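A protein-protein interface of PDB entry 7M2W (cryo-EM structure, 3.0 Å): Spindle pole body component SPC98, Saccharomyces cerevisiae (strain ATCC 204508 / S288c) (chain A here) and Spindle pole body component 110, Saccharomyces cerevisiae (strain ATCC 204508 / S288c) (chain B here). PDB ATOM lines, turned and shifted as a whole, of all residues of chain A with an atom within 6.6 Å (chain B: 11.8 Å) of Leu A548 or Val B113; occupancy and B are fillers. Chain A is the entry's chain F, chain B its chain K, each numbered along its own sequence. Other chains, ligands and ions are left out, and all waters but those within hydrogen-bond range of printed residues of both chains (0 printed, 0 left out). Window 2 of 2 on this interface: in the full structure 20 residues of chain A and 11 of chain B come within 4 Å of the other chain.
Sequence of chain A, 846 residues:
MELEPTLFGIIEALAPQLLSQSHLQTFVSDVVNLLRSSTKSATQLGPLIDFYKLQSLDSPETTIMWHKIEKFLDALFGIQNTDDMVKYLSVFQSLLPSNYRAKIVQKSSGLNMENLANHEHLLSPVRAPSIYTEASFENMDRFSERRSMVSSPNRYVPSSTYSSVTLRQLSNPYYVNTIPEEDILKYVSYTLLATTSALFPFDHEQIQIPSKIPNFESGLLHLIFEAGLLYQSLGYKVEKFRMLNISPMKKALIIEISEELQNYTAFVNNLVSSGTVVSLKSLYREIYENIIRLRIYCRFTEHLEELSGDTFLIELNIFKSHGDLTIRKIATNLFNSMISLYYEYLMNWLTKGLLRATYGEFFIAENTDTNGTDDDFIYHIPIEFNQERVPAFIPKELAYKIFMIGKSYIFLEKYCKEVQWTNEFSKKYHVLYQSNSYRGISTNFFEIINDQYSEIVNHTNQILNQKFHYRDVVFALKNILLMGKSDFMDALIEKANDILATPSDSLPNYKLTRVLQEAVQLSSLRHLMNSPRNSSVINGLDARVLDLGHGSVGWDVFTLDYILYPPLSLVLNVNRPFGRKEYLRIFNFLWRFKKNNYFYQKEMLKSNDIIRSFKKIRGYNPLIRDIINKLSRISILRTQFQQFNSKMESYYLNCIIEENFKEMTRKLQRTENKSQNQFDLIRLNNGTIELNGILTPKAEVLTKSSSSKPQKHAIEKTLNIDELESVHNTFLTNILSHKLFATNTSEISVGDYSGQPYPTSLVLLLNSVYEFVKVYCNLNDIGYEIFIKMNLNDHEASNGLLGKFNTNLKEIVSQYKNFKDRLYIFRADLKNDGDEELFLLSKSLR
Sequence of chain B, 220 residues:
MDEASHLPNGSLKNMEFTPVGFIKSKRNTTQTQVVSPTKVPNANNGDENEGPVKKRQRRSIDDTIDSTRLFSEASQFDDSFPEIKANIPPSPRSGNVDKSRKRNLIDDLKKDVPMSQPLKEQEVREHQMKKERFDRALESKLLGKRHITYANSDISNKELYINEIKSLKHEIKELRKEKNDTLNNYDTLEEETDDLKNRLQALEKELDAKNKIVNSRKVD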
ATOM      1  N   LEU A 546      -2.464 -15.237 -13.168  1.00  0.00           N
ATOM      2  CA  LEU A 546      -3.165 -16.171 -12.300  1.00  0.00           C
ATOM      3  C   LEU A 546      -3.395 -15.568 -10.920  1.00  0.00           C
ATOM      4  O   LEU A 546      -2.933 -14.466 -10.610  1.00  0.00           O
ATOM      5  CB  LEU A 546      -2.384 -17.475 -12.163  1.00  0.00           C
ATOM      6  CG  LEU A 546      -2.408 -18.428 -13.358  1.00  0.00           C
ATOM      7  CD1 LEU A 546      -1.944 -19.810 -12.938  1.00  0.00           C
ATOM      8  CD2 LEU A 546      -3.788 -18.490 -13.984  1.00  0.00           C
ATOM      9  N   ASP A 547      -4.123 -16.308 -10.088  1.00  0.00           N
ATOM     10  CA  ASP A 547      -4.375 -15.908  -8.706  1.00  0.00           C
ATOM     11  C   ASP A 547      -4.105 -17.111  -7.809  1.00  0.00           C
ATOM     12  O   ASP A 547      -5.006 -17.901  -7.521  1.00  0.00           O
ATOM     13  CB  ASP A 547      -5.802 -15.394  -8.547  1.00  0.00           C
ATOM     14  CG  ASP A 547      -6.034 -14.716  -7.211  1.00  0.00           C
ATOM     15  OD1 ASP A 547      -5.093 -14.665  -6.392  1.00  0.00           O
ATOM     16  OD2 ASP A 547      -7.161 -14.230  -6.981  1.00  0.00           O
ATOM     17  N   LEU A 548      -2.857 -17.248  -7.364  1.00  0.00           N
ATOM     18  CA  LEU A 548      -2.464 -18.308  -6.445  1.00  0.00           C
ATOM     19  C   LEU A 548      -2.164 -17.776  -5.049  1.00  0.00           C
ATOM     20  O   LEU A 548      -1.408 -18.403  -4.299  1.00  0.00           O
ATOM     21  CB  LEU A 548      -1.265 -19.075  -6.997  1.00  0.00           C
ATOM     22  CG  LEU A 548      -1.569 -19.984  -8.188  1.00  0.00           C
ATOM     23  CD1 LEU A 548      -0.296 -20.363  -8.916  1.00  0.00           C
ATOM     24  CD2 LEU A 548      -2.308 -21.226  -7.721  1.00  0.00           C
ATOM     25  N   GLY A 549      -2.739 -16.634  -4.689  1.00  0.00           N
ATOM     26  CA  GLY A 549      -2.608 -16.081  -3.354  1.00  0.00           C
ATOM     27  C   GLY A 549      -1.424 -15.144  -3.228  1.00  0.00           C
ATOM     28  O   GLY A 549      -0.737 -14.806  -4.197  1.00  0.00           O
ATOM     29  N   HIS A 550      -1.193 -14.723  -1.991  1.00  0.00           N
ATOM     30  CA  HIS A 550      -0.096 -13.827  -1.666  1.00  0.00           C
ATOM     31  C   HIS A 550       1.217 -14.597  -1.589  1.00  0.00           C
ATOM     32  O   HIS A 550       1.238 -15.810  -1.360  1.00  0.00           O
ATOM     33  CB  HIS A 550      -0.362 -13.105  -0.342  1.00  0.00           C
ATOM     34  CG  HIS A 550       0.675 -12.086   0.010  1.00  0.00           C
ATOM     35  ND1 HIS A 550       1.834 -12.406   0.685  1.00  0.00           N
ATOM     36  CD2 HIS A 550       0.734 -10.755  -0.229  1.00  0.00           C
ATOM     37  CE1 HIS A 550       2.559 -11.314   0.851  1.00  0.00           C
ATOM     38  NE2 HIS A 550       1.914 -10.299   0.307  1.00  0.00           N
ATOM     39  N   GLY A 551       2.317 -13.876  -1.784  1.00  0.00           N
ATOM     40  CA  GLY A 551       3.633 -14.475  -1.768  1.00  0.00           C
ATOM     41  C   GLY A 551       3.979 -15.285  -2.994  1.00  0.00           C
ATOM     42  O   GLY A 551       4.928 -16.075  -2.947  1.00  0.00           O
ATOM     43  N   SER A 552       3.238 -15.121  -4.085  1.00  0.00           N
ATOM     44  CA  SER A 552       3.531 -15.825  -5.319  1.00  0.00           C
ATOM     45  C   SER A 552       4.637 -15.112  -6.091  1.00  0.00           C
ATOM     46  O   SER A 552       5.016 -13.977  -5.792  1.00  0.00           O
ATOM     47  CB  SER A 552       2.273 -15.947  -6.177  1.00  0.00           C
ATOM     48  OG  SER A 552       1.759 -14.669  -6.508  1.00  0.00           O
ATOM     49  N   ASP A 556       5.323 -18.649 -11.539  1.00  0.00           N
ATOM     50  CA  ASP A 556       4.243 -19.611 -11.366  1.00  0.00           C
ATOM     51  C   ASP A 556       2.875 -18.948 -11.466  1.00  0.00           C
ATOM     52  O   ASP A 556       1.868 -19.563 -11.108  1.00  0.00           O
ATOM     53  CB  ASP A 556       4.395 -20.327 -10.020  1.00  0.00           C
ATOM     54  CG  ASP A 556       3.876 -21.754 -10.048  1.00  0.00           C
ATOM     55  OD1 ASP A 556       4.531 -22.632  -9.448  1.00  0.00           O
ATOM     56  OD2 ASP A 556       2.827 -22.008 -10.673  1.00  0.00           O
ATOM     57  N   VAL A 557       2.819 -17.708 -11.941  1.00  0.00           N
ATOM     58  CA  VAL A 557       1.574 -16.968 -12.070  1.00  0.00           C
ATOM     59  C   VAL A 557       1.317 -16.547 -13.513  1.00  0.00           C
ATOM     60  O   VAL A 557       0.192 -16.662 -14.003  1.00  0.00           O
ATOM     61  CB  VAL A 557       1.570 -15.748 -11.123  1.00  0.00           C
ATOM     62  CG1 VAL A 557       0.609 -14.690 -11.610  1.00  0.00           C
ATOM     63  CG2 VAL A 557       1.207 -16.184  -9.714  1.00  0.00           C
ATOM     64  N   LYS A 581     -10.308 -25.639 -19.402  1.00  0.00           N
ATOM     65  CA  LYS A 581      -9.104 -24.830 -19.589  1.00  0.00           C
ATOM     66  C   LYS A 581      -7.902 -25.716 -19.908  1.00  0.00           C
ATOM     67  O   LYS A 581      -6.891 -25.711 -19.205  1.00  0.00           O
ATOM     68  CB  LYS A 581      -8.836 -23.950 -18.366  1.00  0.00           C
ATOM     69  CG  LYS A 581      -9.987 -23.027 -18.008  1.00  0.00           C
ATOM     70  CD  LYS A 581      -9.517 -21.865 -17.154  1.00  0.00           C
ATOM     71  CE  LYS A 581     -10.632 -20.858 -16.935  1.00  0.00           C
ATOM     72  NZ  LYS A 581     -11.669 -21.379 -16.003  1.00  0.00           N
ATOM     73  N   LEU A 584      -4.620 -23.845 -20.764  1.00  0.00           N
ATOM     74  CA  LEU A 584      -3.986 -23.198 -19.617  1.00  0.00           C
ATOM     75  C   LEU A 584      -3.162 -24.186 -18.797  1.00  0.00           C
ATOM     76  O   LEU A 584      -2.013 -23.901 -18.436  1.00  0.00           O
ATOM     77  CB  LEU A 584      -5.044 -22.532 -18.741  1.00  0.00           C
ATOM     78  CG  LEU A 584      -4.584 -21.274 -18.010  1.00  0.00           C
ATOM     79  CD1 LEU A 584      -4.319 -20.155 -19.000  1.00  0.00           C
ATOM     80  CD2 LEU A 584      -5.612 -20.846 -16.980  1.00  0.00           C
ATOM     81  N   ASN A 588       0.849 -24.495 -18.260  1.00  0.00           N
ATOM     82  CA  ASN A 588       1.521 -24.547 -16.962  1.00  0.00           C
ATOM     83  C   ASN A 588       2.536 -25.684 -16.909  1.00  0.00           C
ATOM     84  O   ASN A 588       3.684 -25.495 -16.467  1.00  0.00           O
ATOM     85  CB  ASN A 588       0.495 -24.698 -15.842  1.00  0.00           C
ATOM     86  CG  ASN A 588      -0.002 -23.370 -15.328  1.00  0.00           C
ATOM     87  OD1 ASN A 588       0.629 -22.338 -15.542  1.00  0.00           O
ATOM     88  ND2 ASN A 588      -1.136 -23.385 -14.640  1.00  0.00           N
ATOM     89  N   ASP B 112      -9.186 -23.768 -12.130  1.00  0.00           N
ATOM     90  CA  ASP B 112      -8.753 -24.083 -10.774  1.00  0.00           C
ATOM     91  C   ASP B 112      -8.518 -22.817  -9.956  1.00  0.00           C
ATOM     92  O   ASP B 112      -8.523 -22.854  -8.726  1.00  0.00           O
ATOM     93  CB  ASP B 112      -7.476 -24.925 -10.797  1.00  0.00           C
ATOM     94  CG  ASP B 112      -7.601 -26.157 -11.670  1.00  0.00           C
ATOM     95  OD1 ASP B 112      -7.170 -26.105 -12.841  1.00  0.00           O
ATOM     96  OD2 ASP B 112      -8.127 -27.180 -11.182  1.00  0.00           O
ATOM     97  N   VAL B 113      -8.312 -21.697 -10.643  1.00  0.00           N
ATOM     98  CA  VAL B 113      -7.929 -20.449  -9.985  1.00  0.00           C
ATOM     99  C   VAL B 113      -8.701 -19.304 -10.626  1.00  0.00           C
ATOM    100  O   VAL B 113      -9.128 -19.391 -11.787  1.00  0.00           O
ATOM    101  CB  VAL B 113      -6.405 -20.202 -10.076  1.00  0.00           C
ATOM    102  CG1 VAL B 113      -5.636 -21.274  -9.319  1.00  0.00           C
ATOM    103  CG2 VAL B 113      -5.967 -20.159 -11.530  1.00  0.00           C
ATOM    104  N   PRO B 114      -8.903 -18.208  -9.885  1.00  0.00           N
ATOM    105  CA  PRO B 114      -9.573 -17.022 -10.460  1.00  0.00           C
ATOM    106  C   PRO B 114      -8.592 -16.116 -11.195  1.00  0.00           C
ATOM    107  O   PRO B 114      -8.190 -15.046 -10.725  1.00  0.00           O
ATOM    108  CB  PRO B 114     -10.180 -16.358  -9.222  1.00  0.00           C
ATOM    109  CG  PRO B 114      -9.231 -16.696  -8.129  1.00  0.00           C
ATOM    110  CD  PRO B 114      -8.695 -18.070  -8.432  1.00  0.00           C
ATOM    111  N   MET B 115      -8.189 -16.556 -12.384  1.00  0.00           N
ATOM    112  CA  MET B 115      -7.235 -15.813 -13.189  1.00  0.00           C
ATOM    113  C   MET B 115      -7.803 -14.455 -13.592  1.00  0.00           C
ATOM    114  O   MET B 115      -8.991 -14.168 -13.427  1.00  0.00           O
ATOM    115  CB  MET B 115      -6.857 -16.608 -14.436  1.00  0.00           C
ATOM    116  CG  MET B 115      -8.048 -17.027 -15.272  1.00  0.00           C
ATOM    117  SD  MET B 115      -7.559 -17.790 -16.826  1.00  0.00           S
ATOM    118  CE  MET B 115      -9.081 -17.666 -17.759  1.00  0.00           C
ATOM    119  N   SER B 116      -6.929 -13.614 -14.137  1.00  0.00           N
ATOM    120  CA  SER B 116      -7.326 -12.271 -14.520  1.00  0.00           C
ATOM    121  C   SER B 116      -7.802 -12.244 -15.969  1.00  0.00           C
ATOM    122  O   SER B 116      -7.571 -13.168 -16.753  1.00  0.00           O
ATOM    123  CB  SER B 116      -6.165 -11.297 -14.329  1.00  0.00           C
ATOM    124  OG  SER B 116      -6.523  -9.994 -14.748  1.00  0.00           O
ATOM    125  N   GLN B 117      -8.478 -11.154 -16.322  1.00  0.00           N
ATOM    126  CA  GLN B 117      -8.916 -10.921 -17.691  1.00  0.00           C
ATOM    127  C   GLN B 117      -7.685 -10.742 -18.572  1.00  0.00           C
ATOM    128  O   GLN B 117      -6.574 -10.601 -18.044  1.00  0.00           O
ATOM    129  CB  GLN B 117      -9.833  -9.694 -17.755  1.00  0.00           C
ATOM    130  CG  GLN B 117      -9.132  -8.366 -17.525  1.00  0.00           C
ATOM    131  CD  GLN B 117      -9.093  -7.970 -16.063  1.00  0.00           C
ATOM    132  OE1 GLN B 117      -9.402  -8.772 -15.184  1.00  0.00           O
ATOM    133  NE2 GLN B 117      -8.709  -6.727 -15.795  1.00  0.00           N
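Of the 12 printed residues of chain A, 5 touch a printed residue of chain B.
Printed residues of chain A that touch a printed residue of chain B: Leu A546, Asp A547, Leu A548, Lys A581 and Leu A584.
Hydrophobic or aromatic side chains of chain A that line the printed part of chain B: Leu A546, Leu A548 and Leu A584.
Of the 6 printed residues of chain B, 3 touch a printed residue of chain A.
Printed residues of chain B that touch a printed residue of chain A: Val B113, Pro B114 and Met B115.
Hydrophobic or aromatic side chains of chain B within 4 Å of the printed part of chain A: Val B113, Pro B114 and Met B115.
Among the printed residues, 7 pairs touch across the chains.
Among the printed residues, no Asp or Glu carboxylate lies within 4 Å of a Lys or Arg side-chain nitrogen of the other chain.
The backbone carbonyl oxygen (O) of Val A557 lies within hydrogen-bond range of the backbone NH (N) of Leu A546 (3.1 Å).
Among the printed residues, pairs that only touch across the chains: Asp A547 with Pro B114 (3.3 Å), Leu A584 with Met B115 (3.6 Å), Leu A546 with Met B115 (3.6 Å), Lys A581 with Met B115 (3.6 Å), Leu A546 with Val B113 (3.7 Å), Leu A548 with Val B113 (3.7 Å) and Asp A547 with Val B113 (3.7 Å).
Leu A548 touches one residue of chain B.
Of chain A, only Leu A546 (3.7 Å), Asp A547 (3.7 Å) and Leu A548 (3.7 Å) come within 4 Å of Val B113.
Leu A546 touches just these residues of chain B: Val B113 and Met B115.
Of chain B, only Val B113 and Pro B114 come within 4 Å of Asp A547.
No residue of chain B comes within 4 Å of Gly A549.
Gly A551 touches none of the printed residues of chain B.
Asp A556 touches none of the printed residues of chain B.
No residue of chain B comes within 4 Å of Val A557.
Printed residues of chain A within 4 Å of Pro B114: Asp A547.
Printed residues of chain A within 4 Å of Met B115: Leu A546, Lys A581 and Leu A584.
Of the printed residues of chain B, Lys A581 touches Met B115 (3.6 Å).
Of the printed residues of chain B, Leu A584 touches Met B115.
Asn A588 touches none of the printed residues of chain B.
Ser A552 touches none of the printed residues of chain B.
The nearest residue of chain B that does not touch Leu A548 is Pro B114 (6.0 Å).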
